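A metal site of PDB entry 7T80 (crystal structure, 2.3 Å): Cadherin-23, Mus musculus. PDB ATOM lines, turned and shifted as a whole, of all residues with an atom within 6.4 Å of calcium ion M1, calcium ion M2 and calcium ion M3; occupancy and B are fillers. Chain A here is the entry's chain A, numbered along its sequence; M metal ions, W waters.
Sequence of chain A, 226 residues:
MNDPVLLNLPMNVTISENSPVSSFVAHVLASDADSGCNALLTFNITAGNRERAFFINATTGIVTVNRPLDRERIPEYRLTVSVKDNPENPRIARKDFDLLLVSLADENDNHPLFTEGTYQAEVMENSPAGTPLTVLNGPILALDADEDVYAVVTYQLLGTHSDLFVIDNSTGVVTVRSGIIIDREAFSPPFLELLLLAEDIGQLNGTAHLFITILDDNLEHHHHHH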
ATOM      1  N   GLU A  17      10.368  25.919 -35.857  1.00  0.00           N
ATOM      2  CA  GLU A  17      11.319  24.778 -35.780  1.00  0.00           C
ATOM      3  C   GLU A  17      10.576  23.443 -35.670  1.00  0.00           C
ATOM      4  O   GLU A  17      11.231  22.450 -35.934  1.00  0.00           O
ATOM      5  CB  GLU A  17      12.303  24.946 -34.623  1.00  0.00           C
ATOM      6  CG  GLU A  17      11.683  24.878 -33.244  1.00  0.00           C
ATOM      7  CD  GLU A  17      12.732  24.723 -32.160  1.00  0.00           C
ATOM      8  OE1 GLU A  17      13.683  23.946 -32.439  1.00  0.00           O
ATOM      9  OE2 GLU A  17      12.616  25.376 -31.071  1.00  0.00           O
ATOM     10  N   ASN A  18       9.277  23.407 -35.343  1.00  0.00           N
ATOM     11  CA  ASN A  18       8.509  22.140 -35.266  1.00  0.00           C
ATOM     12  C   ASN A  18       7.768  21.834 -36.585  1.00  0.00           C
ATOM     13  O   ASN A  18       7.054  20.803 -36.608  1.00  0.00           O
ATOM     14  CB  ASN A  18       7.526  22.131 -34.095  1.00  0.00           C
ATOM     15  CG  ASN A  18       8.245  22.067 -32.770  1.00  0.00           C
ATOM     16  OD1 ASN A  18       9.470  21.958 -32.725  1.00  0.00           O
ATOM     17  ND2 ASN A  18       7.499  22.177 -31.694  1.00  0.00           N
ATOM     18  N   LEU A  69      13.693  19.644 -38.087  1.00  0.00           N
ATOM     19  CA  LEU A  69      14.466  20.887 -37.895  1.00  0.00           C
ATOM     20  C   LEU A  69      14.670  21.103 -36.395  1.00  0.00           C
ATOM     21  O   LEU A  69      13.908  20.524 -35.633  1.00  0.00           O
ATOM     22  CB  LEU A  69      13.686  22.048 -38.500  1.00  0.00           C
ATOM     23  CG  LEU A  69      13.292  21.891 -39.961  1.00  0.00           C
ATOM     24  CD1 LEU A  69      12.587  23.128 -40.486  1.00  0.00           C
ATOM     25  CD2 LEU A  69      14.500  21.608 -40.821  1.00  0.00           C
ATOM     26  N   ASP A  70      15.643  21.930 -36.021  1.00  0.00           N
ATOM     27  CA  ASP A  70      16.009  22.189 -34.607  1.00  0.00           C
ATOM     28  C   ASP A  70      16.687  23.558 -34.529  1.00  0.00           C
ATOM     29  O   ASP A  70      17.841  23.666 -34.975  1.00  0.00           O
ATOM     30  CB  ASP A  70      16.896  21.066 -34.069  1.00  0.00           C
ATOM     31  CG  ASP A  70      17.110  21.153 -32.562  1.00  0.00           C
ATOM     32  OD1 ASP A  70      16.492  22.050 -31.919  1.00  0.00           O
ATOM     33  OD2 ASP A  70      17.879  20.332 -32.036  1.00  0.00           O
ATOM     34  N   ARG A  71      15.971  24.569 -34.049  1.00  0.00           N
ATOM     35  CA  ARG A  71      16.527  25.936 -33.959  1.00  0.00           C
ATOM     36  C   ARG A  71      17.824  25.868 -33.147  1.00  0.00           C
ATOM     37  O   ARG A  71      18.740  26.635 -33.445  1.00  0.00           O
ATOM     38  CB  ARG A  71      15.543  26.888 -33.296  1.00  0.00           C
ATOM     39  CG  ARG A  71      15.914  28.359 -33.441  1.00  0.00           C
ATOM     40  CD  ARG A  71      15.356  29.223 -32.299  1.00  0.00           C
ATOM     41  NE  ARG A  71      15.910  28.756 -31.036  1.00  0.00           N
ATOM     42  CZ  ARG A  71      17.138  29.032 -30.616  1.00  0.00           C
ATOM     43  NH1 ARG A  71      17.932  29.847 -31.305  1.00  0.00           N
ATOM     44  NH2 ARG A  71      17.539  28.541 -29.470  1.00  0.00           N
ATOM     45  N   GLU A  72      17.857  24.979 -32.146  1.00  0.00           N
ATOM     46  CA  GLU A  72      18.985  24.791 -31.192  1.00  0.00           C
ATOM     47  C   GLU A  72      20.197  24.190 -31.906  1.00  0.00           C
ATOM     48  O   GLU A  72      21.284  24.279 -31.336  1.00  0.00           O
ATOM     49  CB  GLU A  72      18.551  23.891 -30.031  1.00  0.00           C
ATOM     50  CG  GLU A  72      17.726  24.633 -29.001  1.00  0.00           C
ATOM     51  CD  GLU A  72      16.284  25.018 -29.341  1.00  0.00           C
ATOM     52  OE1 GLU A  72      15.952  26.193 -29.125  1.00  0.00           O
ATOM     53  OE2 GLU A  72      15.448  24.136 -29.703  1.00  0.00           O
ATOM     54  N   ARG A  73      20.015  23.567 -33.088  1.00  0.00           N
ATOM     55  CA  ARG A  73      21.111  22.902 -33.834  1.00  0.00           C
ATOM     56  C   ARG A  73      21.528  23.797 -35.004  1.00  0.00           C
ATOM     57  O   ARG A  73      22.689  24.222 -35.023  1.00  0.00           O
ATOM     58  CB  ARG A  73      20.691  21.508 -34.320  1.00  0.00           C
ATOM     59  CG  ARG A  73      21.826  20.488 -34.327  1.00  0.00           C
ATOM     60  CD  ARG A  73      21.309  19.064 -34.527  1.00  0.00           C
ATOM     61  NE  ARG A  73      21.009  18.935 -35.938  1.00  0.00           N
ATOM     62  CZ  ARG A  73      21.903  18.682 -36.884  1.00  0.00           C
ATOM     63  NH1 ARG A  73      21.534  18.648 -38.151  1.00  0.00           N
ATOM     64  NH2 ARG A  73      23.173  18.459 -36.575  1.00  0.00           N
ATOM     65  N   ALA A 105      11.736  29.961 -36.110  1.00  0.00           N
ATOM     66  CA  ALA A 105      11.136  30.583 -34.908  1.00  0.00           C
ATOM     67  C   ALA A 105      11.241  29.568 -33.774  1.00  0.00           C
ATOM     68  O   ALA A 105      11.009  28.367 -34.015  1.00  0.00           O
ATOM     69  CB  ALA A 105       9.700  30.946 -35.160  1.00  0.00           C
ATOM     70  N   ASP A 106      11.552  30.052 -32.581  1.00  0.00           N
ATOM     71  CA  ASP A 106      11.814  29.208 -31.397  1.00  0.00           C
ATOM     72  C   ASP A 106      10.508  28.613 -30.879  1.00  0.00           C
ATOM     73  O   ASP A 106       9.599  29.379 -30.582  1.00  0.00           O
ATOM     74  CB  ASP A 106      12.466  30.019 -30.277  1.00  0.00           C
ATOM     75  CG  ASP A 106      12.942  29.120 -29.135  1.00  0.00           C
ATOM     76  OD1 ASP A 106      13.435  27.987 -29.413  1.00  0.00           O
ATOM     77  OD2 ASP A 106      12.801  29.554 -27.988  1.00  0.00           O
ATOM     78  N   GLU A 107      10.463  27.294 -30.724  1.00  0.00           N
ATOM     79  CA  GLU A 107       9.408  26.587 -29.956  1.00  0.00           C
ATOM     80  C   GLU A 107       9.976  26.217 -28.574  1.00  0.00           C
ATOM     81  O   GLU A 107      11.222  26.028 -28.415  1.00  0.00           O
ATOM     82  CB  GLU A 107       8.881  25.362 -30.707  1.00  0.00           C
ATOM     83  CG  GLU A 107       8.178  25.661 -32.016  1.00  0.00           C
ATOM     84  CD  GLU A 107       6.939  26.533 -31.907  1.00  0.00           C
ATOM     85  OE1 GLU A 107       6.329  26.541 -30.829  1.00  0.00           O
ATOM     86  OE2 GLU A 107       6.583  27.218 -32.892  1.00  0.00           O
ATOM     87  N   ASN A 108       9.091  26.165 -27.587  1.00  0.00           N
ATOM     88  CA  ASN A 108       9.441  25.780 -26.206  1.00  0.00           C
ATOM     89  C   ASN A 108       9.607  24.262 -26.140  1.00  0.00           C
ATOM     90  O   ASN A 108       8.711  23.649 -25.613  1.00  0.00           O
ATOM     91  CB  ASN A 108       8.364  26.244 -25.207  1.00  0.00           C
ATOM     92  CG  ASN A 108       8.885  26.300 -23.798  1.00  0.00           C
ATOM     93  OD1 ASN A 108      10.074  26.490 -23.586  1.00  0.00           O
ATOM     94  ND2 ASN A 108       8.017  26.154 -22.813  1.00  0.00           N
ATOM     95  N   ASP A 109      10.690  23.703 -26.679  1.00  0.00           N
ATOM     96  CA  ASP A 109      10.903  22.225 -26.723  1.00  0.00           C
ATOM     97  C   ASP A 109      12.031  21.843 -25.750  1.00  0.00           C
ATOM     98  O   ASP A 109      12.483  20.688 -25.785  1.00  0.00           O
ATOM     99  CB  ASP A 109      11.162  21.699 -28.151  1.00  0.00           C
ATOM    100  CG  ASP A 109      12.236  22.414 -28.959  1.00  0.00           C
ATOM    101  OD1 ASP A 109      12.716  23.438 -28.493  1.00  0.00           O
ATOM    102  OD2 ASP A 109      12.571  21.934 -30.095  1.00  0.00           O
ATOM    103  N   ASN A 110      12.489  22.759 -24.919  1.00  0.00           N
ATOM    104  CA  ASN A 110      13.543  22.460 -23.918  1.00  0.00           C
ATOM    105  C   ASN A 110      13.075  22.917 -22.544  1.00  0.00           C
ATOM    106  O   ASN A 110      12.294  23.892 -22.450  1.00  0.00           O
ATOM    107  CB  ASN A 110      14.890  23.106 -24.256  1.00  0.00           C
ATOM    108  CG  ASN A 110      15.477  22.565 -25.543  1.00  0.00           C
ATOM    109  OD1 ASN A 110      16.275  21.636 -25.518  1.00  0.00           O
ATOM    110  ND2 ASN A 110      15.078  23.159 -26.662  1.00  0.00           N
ATOM    111  N   HIS A 111      13.530  22.233 -21.502  1.00  0.00           N
ATOM    112  CA  HIS A 111      13.181  22.547 -20.096  1.00  0.00           C
ATOM    113  C   HIS A 111      14.443  22.875 -19.329  1.00  0.00           C
ATOM    114  O   HIS A 111      15.548  22.490 -19.740  1.00  0.00           O
ATOM    115  CB  HIS A 111      12.322  21.427 -19.468  1.00  0.00           C
ATOM    116  CG  HIS A 111      13.015  20.112 -19.383  1.00  0.00           C
ATOM    117  ND1 HIS A 111      13.766  19.741 -18.258  1.00  0.00           N
ATOM    118  CD2 HIS A 111      13.068  19.087 -20.258  1.00  0.00           C
ATOM    119  CE1 HIS A 111      14.253  18.535 -18.463  1.00  0.00           C
ATOM    120  NE2 HIS A 111      13.844  18.110 -19.681  1.00  0.00           N
ATOM    121  N   PRO A 112      14.312  23.646 -18.232  1.00  0.00           N
ATOM    122  CA  PRO A 112      15.447  23.960 -17.371  1.00  0.00           C
ATOM    123  C   PRO A 112      16.094  22.671 -16.840  1.00  0.00           C
ATOM    124  O   PRO A 112      15.392  21.814 -16.389  1.00  0.00           O
ATOM    125  CB  PRO A 112      14.827  24.782 -16.243  1.00  0.00           C
ATOM    126  CG  PRO A 112      13.507  25.280 -16.809  1.00  0.00           C
ATOM    127  CD  PRO A 112      13.040  24.168 -17.714  1.00  0.00           C
ATOM    128  N   ASP A 144      18.162  26.659 -19.657  1.00  0.00           N
ATOM    129  CA  ASP A 144      17.141  26.263 -20.664  1.00  0.00           C
ATOM    130  C   ASP A 144      17.709  26.667 -22.022  1.00  0.00           C
ATOM    131  O   ASP A 144      17.928  27.884 -22.226  1.00  0.00           O
ATOM    132  CB  ASP A 144      15.771  26.823 -20.290  1.00  0.00           C
ATOM    133  CG  ASP A 144      14.604  26.387 -21.176  1.00  0.00           C
ATOM    134  OD1 ASP A 144      14.715  26.536 -22.415  1.00  0.00           O
ATOM    135  OD2 ASP A 144      13.543  25.992 -20.636  1.00  0.00           O
ATOM    136  N   ALA A 145      17.889  25.674 -22.910  1.00  0.00           N
ATOM    137  CA  ALA A 145      18.496  25.788 -24.246  1.00  0.00           C
ATOM    138  C   ALA A 145      17.614  26.584 -25.228  1.00  0.00           C
ATOM    139  O   ALA A 145      18.069  26.800 -26.336  1.00  0.00           O
ATOM    140  CB  ALA A 145      18.761  24.398 -24.790  1.00  0.00           C
ATOM    141  N   ASP A 146      16.412  27.012 -24.878  1.00  0.00           N
ATOM    142  CA  ASP A 146      15.554  27.755 -25.855  1.00  0.00           C
ATOM    143  C   ASP A 146      16.164  29.156 -26.059  1.00  0.00           C
ATOM    144  O   ASP A 146      17.218  29.417 -25.458  1.00  0.00           O
ATOM    145  CB  ASP A 146      14.101  27.714 -25.410  1.00  0.00           C
ATOM    146  CG  ASP A 146      13.476  26.344 -25.589  1.00  0.00           C
ATOM    147  OD1 ASP A 146      13.586  25.809 -26.731  1.00  0.00           O
ATOM    148  OD2 ASP A 146      12.871  25.841 -24.591  1.00  0.00           O
ATOM    149  N   GLU A 147      15.576  29.988 -26.910  1.00  0.00           N
ATOM    150  CA  GLU A 147      16.255  31.176 -27.503  1.00  0.00           C
ATOM    151  C   GLU A 147      16.327  32.328 -26.492  1.00  0.00           C
ATOM    152  O   GLU A 147      17.453  32.767 -26.213  1.00  0.00           O
ATOM    153  CB  GLU A 147      15.568  31.629 -28.792  1.00  0.00           C
ATOM    154  CG  GLU A 147      16.124  32.947 -29.335  1.00  0.00           C
ATOM    155  CD  GLU A 147      15.816  33.186 -30.803  1.00  0.00           C
ATOM    156  OE1 GLU A 147      14.675  32.921 -31.239  1.00  0.00           O
ATOM    157  OE2 GLU A 147      16.738  33.611 -31.517  1.00  0.00           O
ATOM    158  N   TYR A 150      11.493  31.752 -23.951  1.00  0.00           N
ATOM    159  CA  TYR A 150      11.212  30.356 -23.552  1.00  0.00           C
ATOM    160  C   TYR A 150      12.371  29.782 -22.730  1.00  0.00           C
ATOM    161  O   TYR A 150      12.370  28.597 -22.446  1.00  0.00           O
ATOM    162  CB  TYR A 150      10.906  29.553 -24.820  1.00  0.00           C
ATOM    163  CG  TYR A 150       9.584  29.871 -25.460  1.00  0.00           C
ATOM    164  CD1 TYR A 150       8.457  30.068 -24.681  1.00  0.00           C
ATOM    165  CD2 TYR A 150       9.440  29.908 -26.838  1.00  0.00           C
ATOM    166  CE1 TYR A 150       7.219  30.292 -25.251  1.00  0.00           C
ATOM    167  CE2 TYR A 150       8.205  30.158 -27.427  1.00  0.00           C
ATOM    168  CZ  TYR A 150       7.104  30.362 -26.634  1.00  0.00           C
ATOM    169  OH  TYR A 150       5.862  30.616 -27.169  1.00  0.00           O
ATOM    170  N   ALA A 151      13.382  30.586 -22.413  1.00  0.00           N
ATOM    171  CA  ALA A 151      14.586  30.144 -21.683  1.00  0.00           C
ATOM    172  C   ALA A 151      14.701  30.887 -20.351  1.00  0.00           C
ATOM    173  O   ALA A 151      15.610  30.525 -19.572  1.00  0.00           O
ATOM    174  CB  ALA A 151      15.799  30.358 -22.562  1.00  0.00           C
ATOM    175  N   VAL A 152      13.852  31.886 -20.078  1.00  0.00           N
ATOM    176  CA  VAL A 152      13.837  32.568 -18.755  1.00  0.00           C
ATOM    177  C   VAL A 152      13.379  31.549 -17.705  1.00  0.00           C
ATOM    178  O   VAL A 152      12.308  30.942 -17.863  1.00  0.00           O
ATOM    179  CB  VAL A 152      12.983  33.861 -18.723  1.00  0.00           C
ATOM    180  CG1 VAL A 152      12.894  34.415 -17.301  1.00  0.00           C
ATOM    181  CG2 VAL A 152      13.553  34.916 -19.673  1.00  0.00           C
ATOM    182  N   ASP A 200      10.160  27.305 -16.785  1.00  0.00           N
ATOM    183  CA  ASP A 200      10.128  28.295 -17.890  1.00  0.00           C
ATOM    184  C   ASP A 200       8.696  28.804 -17.963  1.00  0.00           C
ATOM    185  O   ASP A 200       7.868  28.330 -17.179  1.00  0.00           O
ATOM    186  CB  ASP A 200      10.730  27.716 -19.162  1.00  0.00           C
ATOM    187  CG  ASP A 200       9.881  26.716 -19.917  1.00  0.00           C
ATOM    188  OD1 ASP A 200       8.669  26.571 -19.582  1.00  0.00           O
ATOM    189  OD2 ASP A 200      10.424  26.089 -20.855  1.00  0.00           O
ATOM    190  N   ILE A 201       8.407  29.741 -18.863  1.00  0.00           N
ATOM    191  CA  ILE A 201       7.101  30.460 -18.918  1.00  0.00           C
ATOM    192  C   ILE A 201       6.042  29.564 -19.555  1.00  0.00           C
ATOM    193  O   ILE A 201       4.855  29.908 -19.472  1.00  0.00           O
ATOM    194  CB  ILE A 201       7.288  31.820 -19.647  1.00  0.00           C
ATOM    195  CG1 ILE A 201       6.188  32.820 -19.255  1.00  0.00           C
ATOM    196  CG2 ILE A 201       7.409  31.640 -21.162  1.00  0.00           C
ATOM    197  CD1 ILE A 201       6.298  33.338 -17.811  1.00  0.00           C
ATOM    198  N   LEU A 204       7.221  24.244 -18.322  1.00  0.00           N
ATOM    199  CA  LEU A 204       8.144  23.069 -18.396  1.00  0.00           C
ATOM    200  C   LEU A 204       9.151  23.218 -17.248  1.00  0.00           C
ATOM    201  O   LEU A 204       9.727  24.268 -17.108  1.00  0.00           O
ATOM    202  CB  LEU A 204       8.833  23.005 -19.766  1.00  0.00           C
ATOM    203  CG  LEU A 204       7.951  22.884 -21.011  1.00  0.00           C
ATOM    204  CD1 LEU A 204       8.784  22.470 -22.215  1.00  0.00           C
ATOM    205  CD2 LEU A 204       6.819  21.893 -20.821  1.00  0.00           C
HETATM  206 CA    CA M   1      14.468  22.347 -30.831  1.00  0.00          CA
HETATM  207 CA    CA M   2      13.496  25.680 -28.999  1.00  0.00          CA
HETATM  208 CA    CA M   3      12.119  26.283 -22.432  1.00  0.00          CA
HETATM  209  O   HOH W   1      15.304  21.058 -28.984  1.00  0.00           O
HETATM  210  O   HOH W   2      13.844  20.476 -32.121  1.00  0.00           O
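The side-chain carboxylate of Asp 106 lies close to the guanidinium group of Arg 71, at 3.1 Å. OD2 of Asp 106 lies within hydrogen-bond range of N of Glu 147 (3.0 Å). OD1 of Asp 200 lies within hydrogen-bond range of N of Leu 204 (3.0 Å). OD1 of Asp 109 sits close to ND2 of Asn 110. N of Arg 71 sits close to OE1 of Glu 17, at 2.9 Å. OE1 of Glu 72 lies close to NH2 of Arg 71. OE2 of Glu 72 sits close to ND2 of Asn 110, at 3.2 Å. O of Ala 105 is in hydrogen-bond range of N of Glu 17, 3.1 Å away.
Within 4 Å of calcium ion M1: Glu 17, Asp 70, Glu 72 and Asp 109.
The nearest printed residue that does not touch calcium ion M3 is His 111 (4.4 Å).
Calcium ion M1 is bound by OD2 of Asp 109 (2.1 Å), OD1 of Asp 70 (2.3 Å), OE2 of Glu 72 (2.3 Å), water W2 (2.4 Å), OE1 of Glu 17 (2.4 Å) and water W1 (2.4 Å). Slightly farther from calcium ion M1 lies the side-chain carboxylate (OD1) of Asp 109 (3.1 Å).
Calcium ion M2 is bound by the side-chain carboxylate (OE2) of Glu 17, the side-chain carboxylate (OD1) of Asp 146, the side-chain carboxylate (OD1) of Asp 106, the backbone carbonyl oxygen (O) of Glu 107, the side-chain carboxylate (OD1) of Asp 109, the side-chain carboxylate (OE1) of Glu 72 and the side-chain carboxylate (OE2) of Glu 72.
Calcium ion M3 is bound by the side-chain carboxylate (OD2) of Asp 144, the side-chain carboxylate (OD2) of Asp 200, the backbone carbonyl oxygen (O) of Tyr 150, the side-chain carboxylate (OD2) of Asp 146, the side-chain amide oxygen (OD1) of Asn 108, the backbone carbonyl oxygen (O) of Asn 110 and the side-chain carboxylate (OD1) of Asp 144.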
